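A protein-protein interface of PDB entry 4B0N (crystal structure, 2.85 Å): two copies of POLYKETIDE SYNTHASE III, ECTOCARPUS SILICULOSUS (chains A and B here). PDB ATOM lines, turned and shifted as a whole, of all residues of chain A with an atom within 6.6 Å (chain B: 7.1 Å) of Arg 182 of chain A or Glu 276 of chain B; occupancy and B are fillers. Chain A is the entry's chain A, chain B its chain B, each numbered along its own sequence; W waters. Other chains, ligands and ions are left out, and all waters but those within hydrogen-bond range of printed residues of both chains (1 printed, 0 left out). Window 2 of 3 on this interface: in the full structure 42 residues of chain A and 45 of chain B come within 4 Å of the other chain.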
ATOM      1  N   ILE A 175     -25.406 -32.539  -7.540  1.00  0.00           N
ATOM      2  CA  ILE A 175     -26.738 -31.957  -7.370  1.00  0.00           C
ATOM      3  C   ILE A 175     -27.217 -31.388  -8.706  1.00  0.00           C
ATOM      4  O   ILE A 175     -28.402 -31.446  -9.021  1.00  0.00           O
ATOM      5  CB  ILE A 175     -26.776 -30.873  -6.265  1.00  0.00           C
ATOM      6  CG1 ILE A 175     -26.152 -31.396  -4.968  1.00  0.00           C
ATOM      7  CG2 ILE A 175     -28.210 -30.430  -5.993  1.00  0.00           C
ATOM      8  CD1 ILE A 175     -25.760 -30.312  -3.986  1.00  0.00           C
ATOM      9  N   LYS A 176     -26.284 -30.850  -9.487  1.00  0.00           N
ATOM     10  CA  LYS A 176     -26.582 -30.380 -10.837  1.00  0.00           C
ATOM     11  C   LYS A 176     -26.897 -31.539 -11.774  1.00  0.00           C
ATOM     12  O   LYS A 176     -27.975 -31.579 -12.377  1.00  0.00           O
ATOM     13  CB  LYS A 176     -25.422 -29.557 -11.401  1.00  0.00           C
ATOM     14  CG  LYS A 176     -25.620 -28.057 -11.299  1.00  0.00           C
ATOM     15  CD  LYS A 176     -24.674 -27.323 -12.233  1.00  0.00           C
ATOM     16  CE  LYS A 176     -25.246 -25.969 -12.626  1.00  0.00           C
ATOM     17  NZ  LYS A 176     -24.457 -25.305 -13.699  1.00  0.00           N
ATOM     18  N   GLY A 179     -29.693 -34.020 -10.574  1.00  0.00           N
ATOM     19  CA  GLY A 179     -30.889 -33.268 -10.204  1.00  0.00           C
ATOM     20  C   GLY A 179     -31.350 -33.618  -8.800  1.00  0.00           C
ATOM     21  O   GLY A 179     -32.540 -33.828  -8.568  1.00  0.00           O
ATOM     22  N   LEU A 180     -30.399 -33.694  -7.869  1.00  0.00           N
ATOM     23  CA  LEU A 180     -30.688 -33.991  -6.471  1.00  0.00           C
ATOM     24  C   LEU A 180     -31.453 -32.842  -5.827  1.00  0.00           C
ATOM     25  O   LEU A 180     -31.404 -31.714  -6.318  1.00  0.00           O
ATOM     26  CB  LEU A 180     -29.387 -34.238  -5.704  1.00  0.00           C
ATOM     27  CG  LEU A 180     -28.487 -35.404  -6.126  1.00  0.00           C
ATOM     28  CD1 LEU A 180     -27.111 -35.258  -5.491  1.00  0.00           C
ATOM     29  CD2 LEU A 180     -29.104 -36.752  -5.768  1.00  0.00           C
ATOM     30  N   THR A 181     -32.164 -33.133  -4.739  1.00  0.00           N
ATOM     31  CA  THR A 181     -32.869 -32.100  -3.976  1.00  0.00           C
ATOM     32  C   THR A 181     -31.873 -31.073  -3.441  1.00  0.00           C
ATOM     33  O   THR A 181     -30.833 -31.435  -2.889  1.00  0.00           O
ATOM     34  CB  THR A 181     -33.721 -32.686  -2.823  1.00  0.00           C
ATOM     35  OG1 THR A 181     -34.237 -31.623  -2.009  1.00  0.00           O
ATOM     36  CG2 THR A 181     -32.906 -33.648  -1.952  1.00  0.00           C
ATOM     37  N   ARG A 182     -32.198 -29.795  -3.612  1.00  0.00           N
ATOM     38  CA  ARG A 182     -31.252 -28.717  -3.313  1.00  0.00           C
ATOM     39  C   ARG A 182     -31.040 -28.460  -1.822  1.00  0.00           C
ATOM     40  O   ARG A 182     -30.232 -27.610  -1.442  1.00  0.00           O
ATOM     41  CB  ARG A 182     -31.643 -27.433  -4.047  1.00  0.00           C
ATOM     42  CG  ARG A 182     -31.708 -27.604  -5.554  1.00  0.00           C
ATOM     43  CD  ARG A 182     -31.251 -26.348  -6.264  1.00  0.00           C
ATOM     44  NE  ARG A 182     -30.791 -26.639  -7.617  1.00  0.00           N
ATOM     45  CZ  ARG A 182     -29.835 -25.962  -8.246  1.00  0.00           C
ATOM     46  NH1 ARG A 182     -29.219 -24.953  -7.643  1.00  0.00           N
ATOM     47  NH2 ARG A 182     -29.484 -26.300  -9.480  1.00  0.00           N
ATOM     48  N   SER A 183     -31.763 -29.205  -0.987  1.00  0.00           N
ATOM     49  CA  SER A 183     -31.619 -29.121   0.463  1.00  0.00           C
ATOM     50  C   SER A 183     -30.744 -30.251   1.019  1.00  0.00           C
ATOM     51  O   SER A 183     -30.712 -30.482   2.233  1.00  0.00           O
ATOM     52  CB  SER A 183     -32.994 -29.135   1.135  1.00  0.00           C
ATOM     53  OG  SER A 183     -33.486 -30.459   1.264  1.00  0.00           O
ATOM     54  N   VAL A 184     -30.030 -30.942   0.130  1.00  0.00           N
ATOM     55  CA  VAL A 184     -29.222 -32.109   0.510  1.00  0.00           C
ATOM     56  C   VAL A 184     -28.077 -31.747   1.467  1.00  0.00           C
ATOM     57  O   VAL A 184     -27.357 -30.767   1.260  1.00  0.00           O
ATOM     58  CB  VAL A 184     -28.728 -32.915  -0.729  1.00  0.00           C
ATOM     59  CG1 VAL A 184     -27.924 -32.045  -1.682  1.00  0.00           C
ATOM     60  CG2 VAL A 184     -27.922 -34.137  -0.318  1.00  0.00           C
ATOM     61  N   HIS B 271     -30.449 -26.840   8.006  1.00  0.00           N
ATOM     62  CA  HIS B 271     -30.953 -26.571   6.656  1.00  0.00           C
ATOM     63  C   HIS B 271     -29.889 -26.146   5.687  1.00  0.00           C
ATOM     64  O   HIS B 271     -28.901 -25.505   6.060  1.00  0.00           O
ATOM     65  CB  HIS B 271     -32.056 -25.520   6.701  1.00  0.00           C
ATOM     66  CG  HIS B 271     -32.961 -25.532   5.496  1.00  0.00           C
ATOM     67  ND1 HIS B 271     -33.956 -26.425   5.349  1.00  0.00           N
ATOM     68  CD2 HIS B 271     -32.996 -24.716   4.368  1.00  0.00           C
ATOM     69  CE1 HIS B 271     -34.594 -26.198   4.184  1.00  0.00           C
ATOM     70  NE2 HIS B 271     -34.006 -25.152   3.585  1.00  0.00           N
ATOM     71  N   ALA B 272     -30.096 -26.500   4.422  1.00  0.00           N
ATOM     72  CA  ALA B 272     -29.204 -26.101   3.345  1.00  0.00           C
ATOM     73  C   ALA B 272     -30.004 -25.753   2.099  1.00  0.00           C
ATOM     74  O   ALA B 272     -31.113 -26.253   1.905  1.00  0.00           O
ATOM     75  CB  ALA B 272     -28.208 -27.209   3.040  1.00  0.00           C
ATOM     76  N   TRP B 273     -29.446 -24.878   1.268  1.00  0.00           N
ATOM     77  CA  TRP B 273     -30.003 -24.624  -0.057  1.00  0.00           C
ATOM     78  C   TRP B 273     -28.957 -24.215  -1.047  1.00  0.00           C
ATOM     79  O   TRP B 273     -28.335 -23.163  -0.907  1.00  0.00           O
ATOM     80  CB  TRP B 273     -31.117 -23.589  -0.016  1.00  0.00           C
ATOM     81  CG  TRP B 273     -31.917 -23.584  -1.296  1.00  0.00           C
ATOM     82  CD1 TRP B 273     -31.851 -22.665  -2.342  1.00  0.00           C
ATOM     83  CD2 TRP B 273     -32.915 -24.576  -1.722  1.00  0.00           C
ATOM     84  NE1 TRP B 273     -32.724 -23.003  -3.346  1.00  0.00           N
ATOM     85  CE2 TRP B 273     -33.390 -24.137  -3.039  1.00  0.00           C
ATOM     86  CE3 TRP B 273     -33.444 -25.733  -1.162  1.00  0.00           C
ATOM     87  CZ2 TRP B 273     -34.357 -24.842  -3.743  1.00  0.00           C
ATOM     88  CZ3 TRP B 273     -34.418 -26.436  -1.880  1.00  0.00           C
ATOM     89  CH2 TRP B 273     -34.863 -25.999  -3.139  1.00  0.00           C
ATOM     90  N   LEU B 274     -28.759 -25.054  -2.059  1.00  0.00           N
ATOM     91  CA  LEU B 274     -27.852 -24.746  -3.156  1.00  0.00           C
ATOM     92  C   LEU B 274     -28.525 -23.735  -4.083  1.00  0.00           C
ATOM     93  O   LEU B 274     -29.423 -24.087  -4.850  1.00  0.00           O
ATOM     94  CB  LEU B 274     -27.498 -26.020  -3.929  1.00  0.00           C
ATOM     95  CG  LEU B 274     -26.077 -26.264  -4.451  1.00  0.00           C
ATOM     96  CD1 LEU B 274     -26.155 -27.085  -5.726  1.00  0.00           C
ATOM     97  CD2 LEU B 274     -25.288 -24.989  -4.708  1.00  0.00           C
ATOM     98  N   MET B 275     -28.093 -22.480  -3.994  1.00  0.00           N
ATOM     99  CA  MET B 275     -28.699 -21.385  -4.756  1.00  0.00           C
ATOM    100  C   MET B 275     -28.413 -21.535  -6.249  1.00  0.00           C
ATOM    101  O   MET B 275     -27.261 -21.689  -6.653  1.00  0.00           O
ATOM    102  CB  MET B 275     -28.185 -20.030  -4.259  1.00  0.00           C
ATOM    103  CG  MET B 275     -28.362 -19.777  -2.767  1.00  0.00           C
ATOM    104  SD  MET B 275     -27.416 -18.343  -2.210  1.00  0.00           S
ATOM    105  CE  MET B 275     -27.983 -18.189  -0.518  1.00  0.00           C
ATOM    106  N   GLU B 276     -29.470 -21.492  -7.057  1.00  0.00           N
ATOM    107  CA  GLU B 276     -29.358 -21.662  -8.504  1.00  0.00           C
ATOM    108  C   GLU B 276     -28.754 -20.431  -9.192  1.00  0.00           C
ATOM    109  O   GLU B 276     -29.112 -19.292  -8.877  1.00  0.00           O
ATOM    110  CB  GLU B 276     -30.731 -21.997  -9.098  1.00  0.00           C
ATOM    111  CG  GLU B 276     -30.716 -22.374 -10.575  1.00  0.00           C
ATOM    112  CD  GLU B 276     -32.050 -22.910 -11.070  1.00  0.00           C
ATOM    113  OE1 GLU B 276     -33.109 -22.516 -10.534  1.00  0.00           O
ATOM    114  OE2 GLU B 276     -32.038 -23.729 -12.013  1.00  0.00           O
ATOM    115  N   GLY B 277     -27.836 -20.678 -10.127  1.00  0.00           N
ATOM    116  CA  GLY B 277     -27.206 -19.621 -10.922  1.00  0.00           C
ATOM    117  C   GLY B 277     -26.165 -18.804 -10.178  1.00  0.00           C
ATOM    118  O   GLY B 277     -25.888 -17.661 -10.544  1.00  0.00           O
ATOM    119  N   THR B 278     -25.578 -19.399  -9.140  1.00  0.00           N
ATOM    120  CA  THR B 278     -24.611 -18.713  -8.281  1.00  0.00           C
ATOM    121  C   THR B 278     -23.221 -19.355  -8.338  1.00  0.00           C
ATOM    122  O   THR B 278     -22.361 -19.068  -7.498  1.00  0.00           O
ATOM    123  CB  THR B 278     -25.090 -18.690  -6.816  1.00  0.00           C
ATOM    124  OG1 THR B 278     -25.354 -20.028  -6.380  1.00  0.00           O
ATOM    125  CG2 THR B 278     -26.357 -17.859  -6.669  1.00  0.00           C
ATOM    126  N   GLU B 279     -23.004 -20.201  -9.347  1.00  0.00           N
ATOM    127  CA  GLU B 279     -21.794 -21.031  -9.461  1.00  0.00           C
ATOM    128  C   GLU B 279     -20.468 -20.282  -9.298  1.00  0.00           C
ATOM    129  O   GLU B 279     -19.501 -20.845  -8.788  1.00  0.00           O
ATOM    130  CB  GLU B 279     -21.787 -21.812 -10.783  1.00  0.00           C
ATOM    131  CG  GLU B 279     -22.929 -22.810 -10.952  1.00  0.00           C
ATOM    132  CD  GLU B 279     -24.214 -22.182 -11.483  1.00  0.00           C
ATOM    133  OE1 GLU B 279     -24.191 -20.998 -11.884  1.00  0.00           O
ATOM    134  OE2 GLU B 279     -25.255 -22.876 -11.501  1.00  0.00           O
ATOM    135  N   TYR B 302     -26.174 -12.211  -4.870  1.00  0.00           N
ATOM    136  CA  TYR B 302     -26.692 -13.578  -4.760  1.00  0.00           C
ATOM    137  C   TYR B 302     -27.310 -13.836  -3.387  1.00  0.00           C
ATOM    138  O   TYR B 302     -28.380 -14.440  -3.290  1.00  0.00           O
ATOM    139  CB  TYR B 302     -25.594 -14.621  -5.002  1.00  0.00           C
ATOM    140  CG  TYR B 302     -24.955 -14.629  -6.380  1.00  0.00           C
ATOM    141  CD1 TYR B 302     -25.683 -14.293  -7.524  1.00  0.00           C
ATOM    142  CD2 TYR B 302     -23.626 -15.019  -6.538  1.00  0.00           C
ATOM    143  CE1 TYR B 302     -25.092 -14.316  -8.777  1.00  0.00           C
ATOM    144  CE2 TYR B 302     -23.029 -15.045  -7.786  1.00  0.00           C
ATOM    145  CZ  TYR B 302     -23.764 -14.695  -8.900  1.00  0.00           C
ATOM    146  OH  TYR B 302     -23.164 -14.728 -10.136  1.00  0.00           O
ATOM    147  N   ASN B 306     -31.430 -14.476  -2.475  1.00  0.00           N
ATOM    148  CA  ASN B 306     -31.733 -15.865  -2.120  1.00  0.00           C
ATOM    149  C   ASN B 306     -31.927 -16.143  -0.630  1.00  0.00           C
ATOM    150  O   ASN B 306     -32.577 -17.127  -0.265  1.00  0.00           O
ATOM    151  CB  ASN B 306     -30.653 -16.807  -2.664  1.00  0.00           C
ATOM    152  CG  ASN B 306     -30.546 -16.780  -4.179  1.00  0.00           C
ATOM    153  OD1 ASN B 306     -31.551 -16.784  -4.893  1.00  0.00           O
ATOM    154  ND2 ASN B 306     -29.314 -16.770  -4.678  1.00  0.00           N
ATOM    155  N   GLY B 403     -20.817 -22.816  -3.971  1.00  0.00           N
ATOM    156  CA  GLY B 403     -22.001 -23.385  -4.609  1.00  0.00           C
ATOM    157  C   GLY B 403     -22.716 -22.452  -5.573  1.00  0.00           C
ATOM    158  O   GLY B 403     -22.760 -22.726  -6.770  1.00  0.00           O
ATOM    159  N   VAL B 404     -23.285 -21.354  -5.079  1.00  0.00           N
ATOM    160  CA  VAL B 404     -23.241 -20.975  -3.665  1.00  0.00           C
ATOM    161  C   VAL B 404     -24.354 -21.660  -2.872  1.00  0.00           C
ATOM    162  O   VAL B 404     -25.514 -21.688  -3.295  1.00  0.00           O
ATOM    163  CB  VAL B 404     -23.299 -19.437  -3.493  1.00  0.00           C
ATOM    164  CG1 VAL B 404     -23.454 -19.039  -2.032  1.00  0.00           C
ATOM    165  CG2 VAL B 404     -22.049 -18.801  -4.076  1.00  0.00           C
ATOM    166  N   ALA B 406     -26.297 -22.135   1.045  1.00  0.00           N
ATOM    167  CA  ALA B 406     -26.583 -21.539   2.340  1.00  0.00           C
ATOM    168  C   ALA B 406     -26.730 -22.652   3.361  1.00  0.00           C
ATOM    169  O   ALA B 406     -27.694 -23.417   3.322  1.00  0.00           O
ATOM    170  CB  ALA B 406     -27.851 -20.703   2.276  1.00  0.00           C
ATOM    171  N   GLU B 407     -25.749 -22.752   4.251  1.00  0.00           N
ATOM    172  CA  GLU B 407     -25.787 -23.709   5.350  1.00  0.00           C
ATOM    173  C   GLU B 407     -26.221 -23.010   6.628  1.00  0.00           C
ATOM    174  O   GLU B 407     -25.774 -21.896   6.917  1.00  0.00           O
ATOM    175  CB  GLU B 407     -24.413 -24.349   5.543  1.00  0.00           C
ATOM    176  CG  GLU B 407     -24.215 -25.676   4.823  1.00  0.00           C
ATOM    177  CD  GLU B 407     -24.452 -25.610   3.324  1.00  0.00           C
ATOM    178  OE1 GLU B 407     -24.158 -24.565   2.700  1.00  0.00           O
ATOM    179  OE2 GLU B 407     -24.921 -26.620   2.764  1.00  0.00           O
HETATM  180  O   HOH W   1     -25.121 -29.229   3.302  1.00  0.00           O
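The side-chain carboxylate (OE2) of Glu 279 of chain B lies within salt-bridge range of the side-chain amino group (NZ) of Lys 176 of chain A (3.4 Å).
The backbone carbonyl oxygen (O) of Leu 274 of chain B sits at hydrogen-bond distance from the guanidinium group (NH1) of Arg 182 of chain A (2.9 Å).
O of Ile 175 of chain A lies within hydrogen-bond range of N of Leu 180 of chain A (3.2 Å).
The backbone NH (N) of Ala 406 of chain B sits at hydrogen-bond distance from the backbone carbonyl oxygen (O) of Trp 273 of chain B, 3.0 Å away.
OG1 of Thr 278 of chain B is in hydrogen-bond range of O of Met 275 of chain B (2.5 Å).
The side-chain sulfur (SD) of Met 275 of chain B sits close to the side-chain amide nitrogen (ND2) of Asn 306 of chain B.
The backbone NH of Met 275 of chain B sits at hydrogen-bond distance from the backbone carbonyl oxygen of Val 404 of chain B (2.8 Å).
Among the printed residues, merely in contact across the chains: Ile 175 of chain A with Leu 274 of chain B (3.7 Å), Arg 182 of chain A with Ala 272 of chain B (3.7 Å), Arg 182 of chain A with Trp 273 of chain B (3.3 Å), Arg 182 of chain A with Met 275 of chain B (3.8 Å), Arg 182 of chain A with Glu 276 of chain B (3.4 Å), Ser 183 of chain A with Ala 272 of chain B (3.2 Å) and Ser 183 of chain A with Trp 273 of chain B (3.9 Å).
Printed residues of chain B within 4 Å of Ile 175 of chain A: Leu 274.
Of the printed residues of chain B, Lys 176 of chain A touches Glu 279 (3.3 Å).
Of chain B, only Ala 272 (3.7 Å), Trp 273 (3.3 Å), Leu 274 (2.9 Å), Met 275 (3.8 Å) and Glu 276 (3.4 Å) come within 4 Å of Arg 182 of chain A.
Printed residues of chain B within 4 Å of Ser 183 of chain A: Ala 272 (3.2 Å) and Trp 273 (3.9 Å).
Printed residues of chain A within 4 Å of Met 275 of chain B: Arg 182 (3.8 Å).
Of the printed residues of chain A, Glu 276 of chain B touches Arg 182.
Printed residues of chain A within 4 Å of Glu 279 of chain B: Lys 176.
Asn 306 of chain B touches none of the printed residues of chain A.
Val 404 of chain B touches none of the printed residues of chain A.
The nearest residue of chain B that does not touch Arg 182 of chain A is Gly 277 of chain B (5.1 Å).
The nearest printed residue of chain B that does not touch Ser 183 of chain A is His 271 of chain B (4.5 Å).
Of the 15 printed residues of chain B, 6 touch a printed residue of chain A.
Printed residues of chain B that touch a printed residue of chain A: Ala 272, Trp 273, Leu 274, Met 275, Glu 276 and Glu 279.
Among the printed residues, Asp or Glu carboxylates within 4 Å of a Lys or Arg side-chain nitrogen of the other chain: Lys 176 of chain A with Glu 279 of chain B (3.4 Å).
No position is printed for both chains.
Water W1 lies within hydrogen-bond range of OE2 of Glu 407 of chain B (2.7 Å) and O of Val 184 of chain A (3.4 Å).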
